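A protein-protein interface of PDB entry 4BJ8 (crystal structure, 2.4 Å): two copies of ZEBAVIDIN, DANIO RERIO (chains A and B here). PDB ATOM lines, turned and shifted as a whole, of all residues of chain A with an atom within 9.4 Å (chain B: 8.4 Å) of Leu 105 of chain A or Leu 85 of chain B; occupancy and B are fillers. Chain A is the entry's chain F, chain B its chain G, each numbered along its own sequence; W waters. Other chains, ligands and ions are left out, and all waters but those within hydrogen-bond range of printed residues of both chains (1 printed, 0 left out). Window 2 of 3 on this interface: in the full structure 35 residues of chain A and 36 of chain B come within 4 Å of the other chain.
The backbone carbonyl oxygen of Asp 103 of chain A lies within hydrogen-bond range of the side-chain amide nitrogen of Gln 61 of chain B (2.9 Å).
The backbone NH (N) of Ala 102 of chain A sits at hydrogen-bond distance from the side-chain amide oxygen (OE1) of Gln 81 of chain B (3.0 Å).
The side-chain hydroxyl (OG) of Ser 111 of chain A sits close to the backbone carbonyl oxygen (O) of Ala 108 of chain A.
The side-chain amide oxygen of Gln 61 of chain B lies within hydrogen-bond range of the backbone NH of Ile 84 of chain B.
The backbone carbonyl oxygen (O) of Gln 61 of chain B is in hydrogen-bond range of the side-chain amide nitrogen (NE2) of Gln 81 of chain B, at 2.9 Å.
OD1 of Asn 104 of chain A lies close to N of Ala 106 of chain A, at 3.5 Å.
SG of Cys 6 of chain B is disulfide-bonded to SG of Cys 82 of chain B.
The backbone NH of Val 91 of chain B is in hydrogen-bond range of the backbone carbonyl oxygen of Phe 83 of chain B (2.9 Å).
Among the printed residues, merely in contact across the chains: Arg 99 of chain A with Gln 81 of chain B (3.6 Å), Arg 99 of chain A with Lys 93 of chain B (3.7 Å), Val 101 of chain A with Gln 81 of chain B (3.8 Å), Ala 102 of chain A with Phe 83 of chain B (3.9 Å), Asn 104 of chain A with Phe 83 of chain B (3.5 Å), Leu 105 of chain A with Phe 83 of chain B (3.6 Å), Leu 105 of chain A with Leu 85 of chain B (3.96 Å), Leu 105 of chain A with Lys 93 of chain B (3.7 Å) and Ala 108 of chain A with Phe 83 of chain B (3.6 Å).
Of chain B, only Phe 83, Leu 85 and Lys 93 come within 4 Å of Leu 105 of chain A.
Leu 85 of chain B touches just one residue of chain A: Leu 105.
No residue of chain B comes within 4 Å of Ala 106 of chain A.
No residue of chain A comes within 4 Å of Asp 86 of chain B.
No residue of chain A comes within 4 Å of Gly 88 of chain B.
Of the printed residues of chain B, Ala 108 of chain A touches Phe 83 (3.6 Å).
Of the printed residues of chain B, Asp 103 of chain A touches Gln 61 (2.9 Å).
Of the printed residues of chain A, Phe 83 of chain B touches Ala 102 (3.9 Å), Asn 104 (3.5 Å), Leu 105 (3.6 Å) and Ala 108 (3.6 Å).
Printed residues of chain B within 4 Å of Val 101 of chain A: Gln 81 (3.8 Å).
Of the printed residues of chain B, Asn 104 of chain A touches Phe 83 (3.5 Å).
Leu 92 of chain B touches none of the printed residues of chain A.
The nearest residue of chain B that does not touch Leu 105 of chain A is Val 91 of chain B (4.5 Å).
Along chain A the printed residues that touch a printed residue of chain B span positions 99 to 108.
Hydrophobic or aromatic side chains of chain B within 4 Å of the printed part of chain A: Phe 83 and Leu 85.
Among the printed residues, 11 pairs touch across the chains.
Among the printed residues, no Asp or Glu carboxylate lies within 4 Å of a Lys or Arg side-chain nitrogen of the other chain.
No position is printed for both chains.
Water W1 lies within hydrogen-bond range of the side-chain amide oxygen of Gln 81 of chain B and the guanidinium group of Arg 99 of chain A.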
ATOM      1  N   ARG A  99      18.929 -17.980  -9.206  1.00  0.00           N
ATOM      2  CA  ARG A  99      19.219 -18.333 -10.591  1.00  0.00           C
ATOM      3  C   ARG A  99      20.454 -19.235 -10.654  1.00  0.00           C
ATOM      4  O   ARG A  99      21.474 -18.904 -10.069  1.00  0.00           O
ATOM      5  CB  ARG A  99      19.393 -17.099 -11.497  1.00  0.00           C
ATOM      6  CG  ARG A  99      19.553 -17.449 -12.979  1.00  0.00           C
ATOM      7  CD  ARG A  99      19.404 -16.252 -13.879  1.00  0.00           C
ATOM      8  NE  ARG A  99      18.087 -16.183 -14.542  1.00  0.00           N
ATOM      9  CZ  ARG A  99      17.765 -16.761 -15.700  1.00  0.00           C
ATOM     10  NH1 ARG A  99      18.623 -17.452 -16.408  1.00  0.00           N
ATOM     11  NH2 ARG A  99      16.549 -16.638 -16.164  1.00  0.00           N
ATOM     12  N   VAL A 101      23.380 -21.303 -13.102  1.00  0.00           N
ATOM     13  CA  VAL A 101      24.099 -21.146 -14.373  1.00  0.00           C
ATOM     14  C   VAL A 101      23.457 -22.080 -15.413  1.00  0.00           C
ATOM     15  O   VAL A 101      23.172 -23.250 -15.125  1.00  0.00           O
ATOM     16  CB  VAL A 101      25.641 -21.394 -14.248  1.00  0.00           C
ATOM     17  CG1 VAL A 101      26.381 -21.131 -15.574  1.00  0.00           C
ATOM     18  CG2 VAL A 101      26.254 -20.477 -13.196  1.00  0.00           C
ATOM     19  N   ALA A 102      23.188 -21.526 -16.592  1.00  0.00           N
ATOM     20  CA  ALA A 102      22.759 -22.288 -17.776  1.00  0.00           C
ATOM     21  C   ALA A 102      23.808 -22.146 -18.891  1.00  0.00           C
ATOM     22  O   ALA A 102      24.462 -21.102 -19.027  1.00  0.00           O
ATOM     23  CB  ALA A 102      21.422 -21.787 -18.291  1.00  0.00           C
ATOM     24  N   ASP A 103      23.904 -23.163 -19.731  1.00  0.00           N
ATOM     25  CA  ASP A 103      24.829 -23.115 -20.858  1.00  0.00           C
ATOM     26  C   ASP A 103      24.388 -22.186 -21.986  1.00  0.00           C
ATOM     27  O   ASP A 103      25.227 -21.624 -22.680  1.00  0.00           O
ATOM     28  CB  ASP A 103      25.080 -24.545 -21.351  1.00  0.00           C
ATOM     29  CG  ASP A 103      25.833 -25.360 -20.321  1.00  0.00           C
ATOM     30  OD1 ASP A 103      26.750 -24.809 -19.679  1.00  0.00           O
ATOM     31  OD2 ASP A 103      25.506 -26.533 -20.114  1.00  0.00           O
ATOM     32  N   ASN A 104      23.083 -21.987 -22.156  1.00  0.00           N
ATOM     33  CA  ASN A 104      22.583 -21.094 -23.226  1.00  0.00           C
ATOM     34  C   ASN A 104      21.129 -20.716 -23.015  1.00  0.00           C
ATOM     35  O   ASN A 104      20.492 -21.188 -22.070  1.00  0.00           O
ATOM     36  CB  ASN A 104      22.761 -21.753 -24.595  1.00  0.00           C
ATOM     37  CG  ASN A 104      22.182 -23.144 -24.641  1.00  0.00           C
ATOM     38  OD1 ASN A 104      20.973 -23.321 -24.654  1.00  0.00           O
ATOM     39  ND2 ASN A 104      23.042 -24.140 -24.639  1.00  0.00           N
ATOM     40  N   LEU A 105      20.605 -19.867 -23.886  1.00  0.00           N
ATOM     41  CA  LEU A 105      19.288 -19.279 -23.668  1.00  0.00           C
ATOM     42  C   LEU A 105      18.212 -20.340 -23.517  1.00  0.00           C
ATOM     43  O   LEU A 105      17.437 -20.324 -22.553  1.00  0.00           O
ATOM     44  CB  LEU A 105      18.915 -18.345 -24.822  1.00  0.00           C
ATOM     45  CG  LEU A 105      17.543 -17.684 -24.639  1.00  0.00           C
ATOM     46  CD1 LEU A 105      17.549 -16.697 -23.476  1.00  0.00           C
ATOM     47  CD2 LEU A 105      17.094 -16.995 -25.912  1.00  0.00           C
ATOM     48  N   ALA A 106      18.175 -21.243 -24.491  1.00  0.00           N
ATOM     49  CA  ALA A 106      17.170 -22.287 -24.588  1.00  0.00           C
ATOM     50  C   ALA A 106      17.130 -23.179 -23.363  1.00  0.00           C
ATOM     51  O   ALA A 106      16.062 -23.569 -22.918  1.00  0.00           O
ATOM     52  CB  ALA A 106      17.406 -23.147 -25.827  1.00  0.00           C
ATOM     53  N   SER A 107      18.282 -23.513 -22.818  1.00  0.00           N
ATOM     54  CA  SER A 107      18.301 -24.463 -21.713  1.00  0.00           C
ATOM     55  C   SER A 107      18.233 -23.770 -20.353  1.00  0.00           C
ATOM     56  O   SER A 107      18.389 -24.438 -19.357  1.00  0.00           O
ATOM     57  CB  SER A 107      19.518 -25.416 -21.814  1.00  0.00           C
ATOM     58  OG  SER A 107      20.693 -24.706 -22.066  1.00  0.00           O
ATOM     59  N   ALA A 108      17.966 -22.456 -20.337  1.00  0.00           N
ATOM     60  CA  ALA A 108      17.822 -21.633 -19.130  1.00  0.00           C
ATOM     61  C   ALA A 108      16.354 -21.508 -18.591  1.00  0.00           C
ATOM     62  O   ALA A 108      16.087 -20.832 -17.582  1.00  0.00           O
ATOM     63  CB  ALA A 108      18.369 -20.250 -19.413  1.00  0.00           C
ATOM     64  N   TRP A 109      15.432 -22.203 -19.258  1.00  0.00           N
ATOM     65  CA  TRP A 109      14.000 -22.092 -19.002  1.00  0.00           C
ATOM     66  C   TRP A 109      13.624 -22.489 -17.618  1.00  0.00           C
ATOM     67  O   TRP A 109      12.604 -22.029 -17.128  1.00  0.00           O
ATOM     68  CB  TRP A 109      13.198 -22.966 -19.977  1.00  0.00           C
ATOM     69  CG  TRP A 109      13.410 -24.439 -19.795  1.00  0.00           C
ATOM     70  CD1 TRP A 109      14.282 -25.244 -20.505  1.00  0.00           C
ATOM     71  CD2 TRP A 109      12.728 -25.311 -18.870  1.00  0.00           C
ATOM     72  NE1 TRP A 109      14.176 -26.542 -20.071  1.00  0.00           N
ATOM     73  CE2 TRP A 109      13.238 -26.617 -19.074  1.00  0.00           C
ATOM     74  CE3 TRP A 109      11.745 -25.116 -17.884  1.00  0.00           C
ATOM     75  CZ2 TRP A 109      12.811 -27.709 -18.323  1.00  0.00           C
ATOM     76  CZ3 TRP A 109      11.311 -26.203 -17.152  1.00  0.00           C
ATOM     77  CH2 TRP A 109      11.850 -27.487 -17.371  1.00  0.00           C
ATOM     78  N   GLY A 110      14.398 -23.412 -17.038  1.00  0.00           N
ATOM     79  CA  GLY A 110      14.151 -23.960 -15.707  1.00  0.00           C
ATOM     80  C   GLY A 110      15.193 -23.559 -14.687  1.00  0.00           C
ATOM     81  O   GLY A 110      15.382 -24.229 -13.695  1.00  0.00           O
ATOM     82  N   SER A 111      15.829 -22.420 -14.901  1.00  0.00           N
ATOM     83  CA  SER A 111      16.981 -22.032 -14.102  1.00  0.00           C
ATOM     84  C   SER A 111      16.631 -21.085 -12.969  1.00  0.00           C
ATOM     85  O   SER A 111      17.514 -20.654 -12.271  1.00  0.00           O
ATOM     86  CB  SER A 111      18.057 -21.386 -14.998  1.00  0.00           C
ATOM     87  OG  SER A 111      18.646 -22.335 -15.885  1.00  0.00           O
ATOM     88  N   SER B   4      33.700 -15.313 -28.121  1.00  0.00           N
ATOM     89  CA  SER B   4      32.459 -14.479 -28.021  1.00  0.00           C
ATOM     90  C   SER B   4      31.784 -14.623 -26.624  1.00  0.00           C
ATOM     91  O   SER B   4      31.528 -15.739 -26.116  1.00  0.00           O
ATOM     92  CB  SER B   4      31.475 -14.808 -29.164  1.00  0.00           C
ATOM     93  OG  SER B   4      30.917 -13.631 -29.725  1.00  0.00           O
ATOM     94  N   SER B   5      31.510 -13.467 -26.022  1.00  0.00           N
ATOM     95  CA  SER B   5      31.002 -13.387 -24.672  1.00  0.00           C
ATOM     96  C   SER B   5      29.781 -12.477 -24.619  1.00  0.00           C
ATOM     97  O   SER B   5      29.347 -11.935 -25.626  1.00  0.00           O
ATOM     98  CB  SER B   5      32.090 -12.830 -23.770  1.00  0.00           C
ATOM     99  OG  SER B   5      32.149 -11.424 -23.900  1.00  0.00           O
ATOM    100  N   CYS B   6      29.205 -12.331 -23.438  1.00  0.00           N
ATOM    101  CA  CYS B   6      28.113 -11.395 -23.259  1.00  0.00           C
ATOM    102  C   CYS B   6      28.688 -10.380 -22.319  1.00  0.00           C
ATOM    103  O   CYS B   6      29.381 -10.744 -21.368  1.00  0.00           O
ATOM    104  CB  CYS B   6      26.857 -12.066 -22.663  1.00  0.00           C
ATOM    105  SG  CYS B   6      25.344 -11.058 -22.748  1.00  0.00           S
ATOM    106  N   GLN B  61      29.392 -15.915 -20.159  1.00  0.00           N
ATOM    107  CA  GLN B  61      27.959 -15.612 -20.128  1.00  0.00           C
ATOM    108  C   GLN B  61      27.588 -15.400 -18.689  1.00  0.00           C
ATOM    109  O   GLN B  61      27.092 -16.315 -18.055  1.00  0.00           O
ATOM    110  CB  GLN B  61      27.186 -16.775 -20.736  1.00  0.00           C
ATOM    111  CG  GLN B  61      27.341 -16.801 -22.224  1.00  0.00           C
ATOM    112  CD  GLN B  61      26.522 -17.851 -22.909  1.00  0.00           C
ATOM    113  OE1 GLN B  61      25.732 -17.529 -23.807  1.00  0.00           O
ATOM    114  NE2 GLN B  61      26.709 -19.108 -22.528  1.00  0.00           N
ATOM    115  N   GLN B  81      20.935 -14.059 -16.331  1.00  0.00           N
ATOM    116  CA  GLN B  81      22.118 -14.377 -17.079  1.00  0.00           C
ATOM    117  C   GLN B  81      22.174 -13.638 -18.412  1.00  0.00           C
ATOM    118  O   GLN B  81      21.136 -13.396 -19.027  1.00  0.00           O
ATOM    119  CB  GLN B  81      22.178 -15.887 -17.311  1.00  0.00           C
ATOM    120  CG  GLN B  81      23.588 -16.351 -17.650  1.00  0.00           C
ATOM    121  CD  GLN B  81      23.799 -17.845 -17.534  1.00  0.00           C
ATOM    122  OE1 GLN B  81      22.874 -18.613 -17.275  1.00  0.00           O
ATOM    123  NE2 GLN B  81      25.028 -18.268 -17.751  1.00  0.00           N
ATOM    124  N   CYS B  82      23.408 -13.310 -18.837  1.00  0.00           N
ATOM    125  CA  CYS B  82      23.756 -12.567 -20.095  1.00  0.00           C
ATOM    126  C   CYS B  82      24.150 -13.629 -21.125  1.00  0.00           C
ATOM    127  O   CYS B  82      25.208 -14.280 -20.989  1.00  0.00           O
ATOM    128  CB  CYS B  82      24.924 -11.585 -19.819  1.00  0.00           C
ATOM    129  SG  CYS B  82      25.222 -10.156 -20.939  1.00  0.00           S
ATOM    130  N   PHE B  83      23.288 -13.852 -22.114  1.00  0.00           N
ATOM    131  CA  PHE B  83      23.544 -14.847 -23.153  1.00  0.00           C
ATOM    132  C   PHE B  83      23.968 -14.167 -24.445  1.00  0.00           C
ATOM    133  O   PHE B  83      23.490 -13.076 -24.773  1.00  0.00           O
ATOM    134  CB  PHE B  83      22.308 -15.714 -23.417  1.00  0.00           C
ATOM    135  CG  PHE B  83      21.883 -16.514 -22.239  1.00  0.00           C
ATOM    136  CD1 PHE B  83      22.624 -17.630 -21.844  1.00  0.00           C
ATOM    137  CD2 PHE B  83      20.770 -16.130 -21.477  1.00  0.00           C
ATOM    138  CE1 PHE B  83      22.264 -18.362 -20.732  1.00  0.00           C
ATOM    139  CE2 PHE B  83      20.401 -16.877 -20.364  1.00  0.00           C
ATOM    140  CZ  PHE B  83      21.157 -17.987 -19.987  1.00  0.00           C
ATOM    141  N   ILE B  84      24.867 -14.806 -25.178  1.00  0.00           N
ATOM    142  CA  ILE B  84      25.239 -14.342 -26.530  1.00  0.00           C
ATOM    143  C   ILE B  84      24.617 -15.350 -27.481  1.00  0.00           C
ATOM    144  O   ILE B  84      24.777 -16.567 -27.330  1.00  0.00           O
ATOM    145  CB  ILE B  84      26.770 -14.173 -26.709  1.00  0.00           C
ATOM    146  CG1 ILE B  84      27.169 -13.896 -28.189  1.00  0.00           C
ATOM    147  CG2 ILE B  84      27.514 -15.378 -26.135  1.00  0.00           C
ATOM    148  CD1 ILE B  84      26.762 -12.540 -28.760  1.00  0.00           C
ATOM    149  N   LEU B  85      23.835 -14.826 -28.408  1.00  0.00           N
ATOM    150  CA  LEU B  85      23.038 -15.659 -29.309  1.00  0.00           C
ATOM    151  C   LEU B  85      23.834 -16.010 -30.576  1.00  0.00           C
ATOM    152  O   LEU B  85      24.949 -15.515 -30.797  1.00  0.00           O
ATOM    153  CB  LEU B  85      21.688 -14.959 -29.656  1.00  0.00           C
ATOM    154  CG  LEU B  85      20.680 -14.630 -28.524  1.00  0.00           C
ATOM    155  CD1 LEU B  85      19.317 -14.167 -29.034  1.00  0.00           C
ATOM    156  CD2 LEU B  85      20.479 -15.812 -27.593  1.00  0.00           C
ATOM    157  N   ASP B  86      23.249 -16.877 -31.395  1.00  0.00           N
ATOM    158  CA  ASP B  86      23.864 -17.314 -32.645  1.00  0.00           C
ATOM    159  C   ASP B  86      23.993 -16.165 -33.622  1.00  0.00           C
ATOM    160  O   ASP B  86      24.956 -16.098 -34.375  1.00  0.00           O
ATOM    161  CB  ASP B  86      23.043 -18.440 -33.259  1.00  0.00           C
ATOM    162  CG  ASP B  86      22.959 -19.642 -32.344  1.00  0.00           C
ATOM    163  OD1 ASP B  86      23.990 -19.953 -31.707  1.00  0.00           O
ATOM    164  OD2 ASP B  86      21.879 -20.261 -32.249  1.00  0.00           O
ATOM    165  N   ASP B  87      23.046 -15.238 -33.576  1.00  0.00           N
ATOM    166  CA  ASP B  87      23.046 -14.103 -34.493  1.00  0.00           C
ATOM    167  C   ASP B  87      23.908 -12.939 -34.004  1.00  0.00           C
ATOM    168  O   ASP B  87      23.786 -11.829 -34.524  1.00  0.00           O
ATOM    169  CB  ASP B  87      21.595 -13.650 -34.800  1.00  0.00           C
ATOM    170  CG  ASP B  87      20.904 -12.974 -33.618  1.00  0.00           C
ATOM    171  OD1 ASP B  87      21.428 -11.967 -33.113  1.00  0.00           O
ATOM    172  OD2 ASP B  87      19.812 -13.435 -33.208  1.00  0.00           O
ATOM    173  N   GLY B  88      24.765 -13.179 -33.011  1.00  0.00           N
ATOM    174  CA  GLY B  88      25.605 -12.121 -32.456  1.00  0.00           C
ATOM    175  C   GLY B  88      24.968 -11.205 -31.411  1.00  0.00           C
ATOM    176  O   GLY B  88      25.673 -10.395 -30.792  1.00  0.00           O
ATOM    177  N   ALA B  89      23.657 -11.317 -31.177  1.00  0.00           N
ATOM    178  CA  ALA B  89      22.995 -10.443 -30.186  1.00  0.00           C
ATOM    179  C   ALA B  89      23.182 -10.932 -28.740  1.00  0.00           C
ATOM    180  O   ALA B  89      23.217 -12.150 -28.443  1.00  0.00           O
ATOM    181  CB  ALA B  89      21.517 -10.267 -30.495  1.00  0.00           C
ATOM    182  N   GLN B  90      23.314  -9.939 -27.860  1.00  0.00           N
ATOM    183  CA  GLN B  90      23.471 -10.126 -26.423  1.00  0.00           C
ATOM    184  C   GLN B  90      22.110  -9.898 -25.792  1.00  0.00           C
ATOM    185  O   GLN B  90      21.510  -8.842 -25.955  1.00  0.00           O
ATOM    186  CB  GLN B  90      24.484  -9.125 -25.886  1.00  0.00           C
ATOM    187  CG  GLN B  90      25.884  -9.255 -26.513  1.00  0.00           C
ATOM    188  CD  GLN B  90      26.798  -8.106 -26.127  1.00  0.00           C
ATOM    189  OE1 GLN B  90      27.546  -8.191 -25.168  1.00  0.00           O
ATOM    190  NE2 GLN B  90      26.687  -6.996 -26.843  1.00  0.00           N
ATOM    191  N   VAL B  91      21.590 -10.916 -25.122  1.00  0.00           N
ATOM    192  CA  VAL B  91      20.288 -10.801 -24.444  1.00  0.00           C
ATOM    193  C   VAL B  91      20.496 -11.000 -22.960  1.00  0.00           C
ATOM    194  O   VAL B  91      21.056 -12.008 -22.559  1.00  0.00           O
ATOM    195  CB  VAL B  91      19.200 -11.797 -24.985  1.00  0.00           C
ATOM    196  CG1 VAL B  91      19.729 -13.210 -25.202  1.00  0.00           C
ATOM    197  CG2 VAL B  91      18.002 -11.861 -24.049  1.00  0.00           C
ATOM    198  N   LEU B  92      20.039 -10.046 -22.157  1.00  0.00           N
ATOM    199  CA  LEU B  92      20.015 -10.181 -20.699  1.00  0.00           C
ATOM    200  C   LEU B  92      18.646 -10.718 -20.202  1.00  0.00           C
ATOM    201  O   LEU B  92      17.641 -10.000 -20.181  1.00  0.00           O
ATOM    202  CB  LEU B  92      20.335  -8.824 -20.079  1.00  0.00           C
ATOM    203  CG  LEU B  92      20.469  -8.684 -18.571  1.00  0.00           C
ATOM    204  CD1 LEU B  92      21.197  -9.867 -17.953  1.00  0.00           C
ATOM    205  CD2 LEU B  92      21.124  -7.352 -18.178  1.00  0.00           C
ATOM    206  N   LYS B  93      18.634 -11.980 -19.785  1.00  0.00           N
ATOM    207  CA  LYS B  93      17.413 -12.692 -19.371  1.00  0.00           C
ATOM    208  C   LYS B  93      17.238 -12.662 -17.861  1.00  0.00           C
ATOM    209  O   LYS B  93      17.984 -13.342 -17.162  1.00  0.00           O
ATOM    210  CB  LYS B  93      17.539 -14.150 -19.820  1.00  0.00           C
ATOM    211  CG  LYS B  93      16.341 -15.050 -19.578  1.00  0.00           C
ATOM    212  CD  LYS B  93      15.532 -15.191 -20.832  1.00  0.00           C
ATOM    213  CE  LYS B  93      14.656 -16.411 -20.823  1.00  0.00           C
ATOM    214  NZ  LYS B  93      13.839 -16.379 -22.071  1.00  0.00           N
ATOM    215  N   THR B  94      16.253 -11.920 -17.348  1.00  0.00           N
ATOM    216  CA  THR B  94      16.060 -11.807 -15.893  1.00  0.00           C
ATOM    217  C   THR B  94      14.673 -12.219 -15.430  1.00  0.00           C
ATOM    218  O   THR B  94      13.750 -12.299 -16.239  1.00  0.00           O
ATOM    219  CB  THR B  94      16.237 -10.363 -15.418  1.00  0.00           C
ATOM    220  OG1 THR B  94      15.230  -9.525 -16.022  1.00  0.00           O
ATOM    221  CG2 THR B  94      17.650  -9.854 -15.760  1.00  0.00           C
ATOM    222  N   GLU B 116       9.004 -11.527 -15.629  1.00  0.00           N
ATOM    223  CA  GLU B 116      10.215 -11.687 -16.441  1.00  0.00           C
ATOM    224  C   GLU B 116      10.562 -10.396 -17.179  1.00  0.00           C
ATOM    225  O   GLU B 116       9.683  -9.716 -17.680  1.00  0.00           O
ATOM    226  CB  GLU B 116      10.062 -12.804 -17.465  1.00  0.00           C
ATOM    227  CG  GLU B 116      11.414 -13.212 -18.037  1.00  0.00           C
ATOM    228  CD  GLU B 116      11.368 -14.357 -19.014  1.00  0.00           C
ATOM    229  OE1 GLU B 116      10.428 -14.441 -19.826  1.00  0.00           O
ATOM    230  OE2 GLU B 116      12.293 -15.185 -18.994  1.00  0.00           O
ATOM    231  N   ILE B 118      13.190  -9.263 -20.280  1.00  0.00           N
ATOM    232  CA  ILE B 118      14.202  -9.542 -21.277  1.00  0.00           C
ATOM    233  C   ILE B 118      14.788  -8.207 -21.763  1.00  0.00           C
ATOM    234  O   ILE B 118      14.074  -7.376 -22.336  1.00  0.00           O
ATOM    235  CB  ILE B 118      13.618 -10.373 -22.437  1.00  0.00           C
ATOM    236  CG1 ILE B 118      13.004 -11.694 -21.898  1.00  0.00           C
ATOM    237  CG2 ILE B 118      14.714 -10.750 -23.413  1.00  0.00           C
ATOM    238  CD1 ILE B 118      12.233 -12.516 -22.906  1.00  0.00           C
ATOM    239  N   PHE B 120      17.505  -6.055 -24.090  1.00  0.00           N
ATOM    240  CA  PHE B 120      18.357  -6.077 -25.289  1.00  0.00           C
ATOM    241  C   PHE B 120      19.242  -4.846 -25.213  1.00  0.00           C
ATOM    242  O   PHE B 120      18.869  -3.868 -24.592  1.00  0.00           O
ATOM    243  CB  PHE B 120      17.556  -6.075 -26.595  1.00  0.00           C
ATOM    244  CG  PHE B 120      16.724  -7.313 -26.809  1.00  0.00           C
ATOM    245  CD1 PHE B 120      17.324  -8.544 -27.069  1.00  0.00           C
ATOM    246  CD2 PHE B 120      15.320  -7.248 -26.785  1.00  0.00           C
ATOM    247  CE1 PHE B 120      16.550  -9.685 -27.276  1.00  0.00           C
ATOM    248  CE2 PHE B 120      14.548  -8.382 -26.997  1.00  0.00           C
ATOM    249  CZ  PHE B 120      15.162  -9.603 -27.235  1.00  0.00           C
HETATM  250  O   HOH W   1      20.666 -18.858 -16.281  1.00  0.00           O
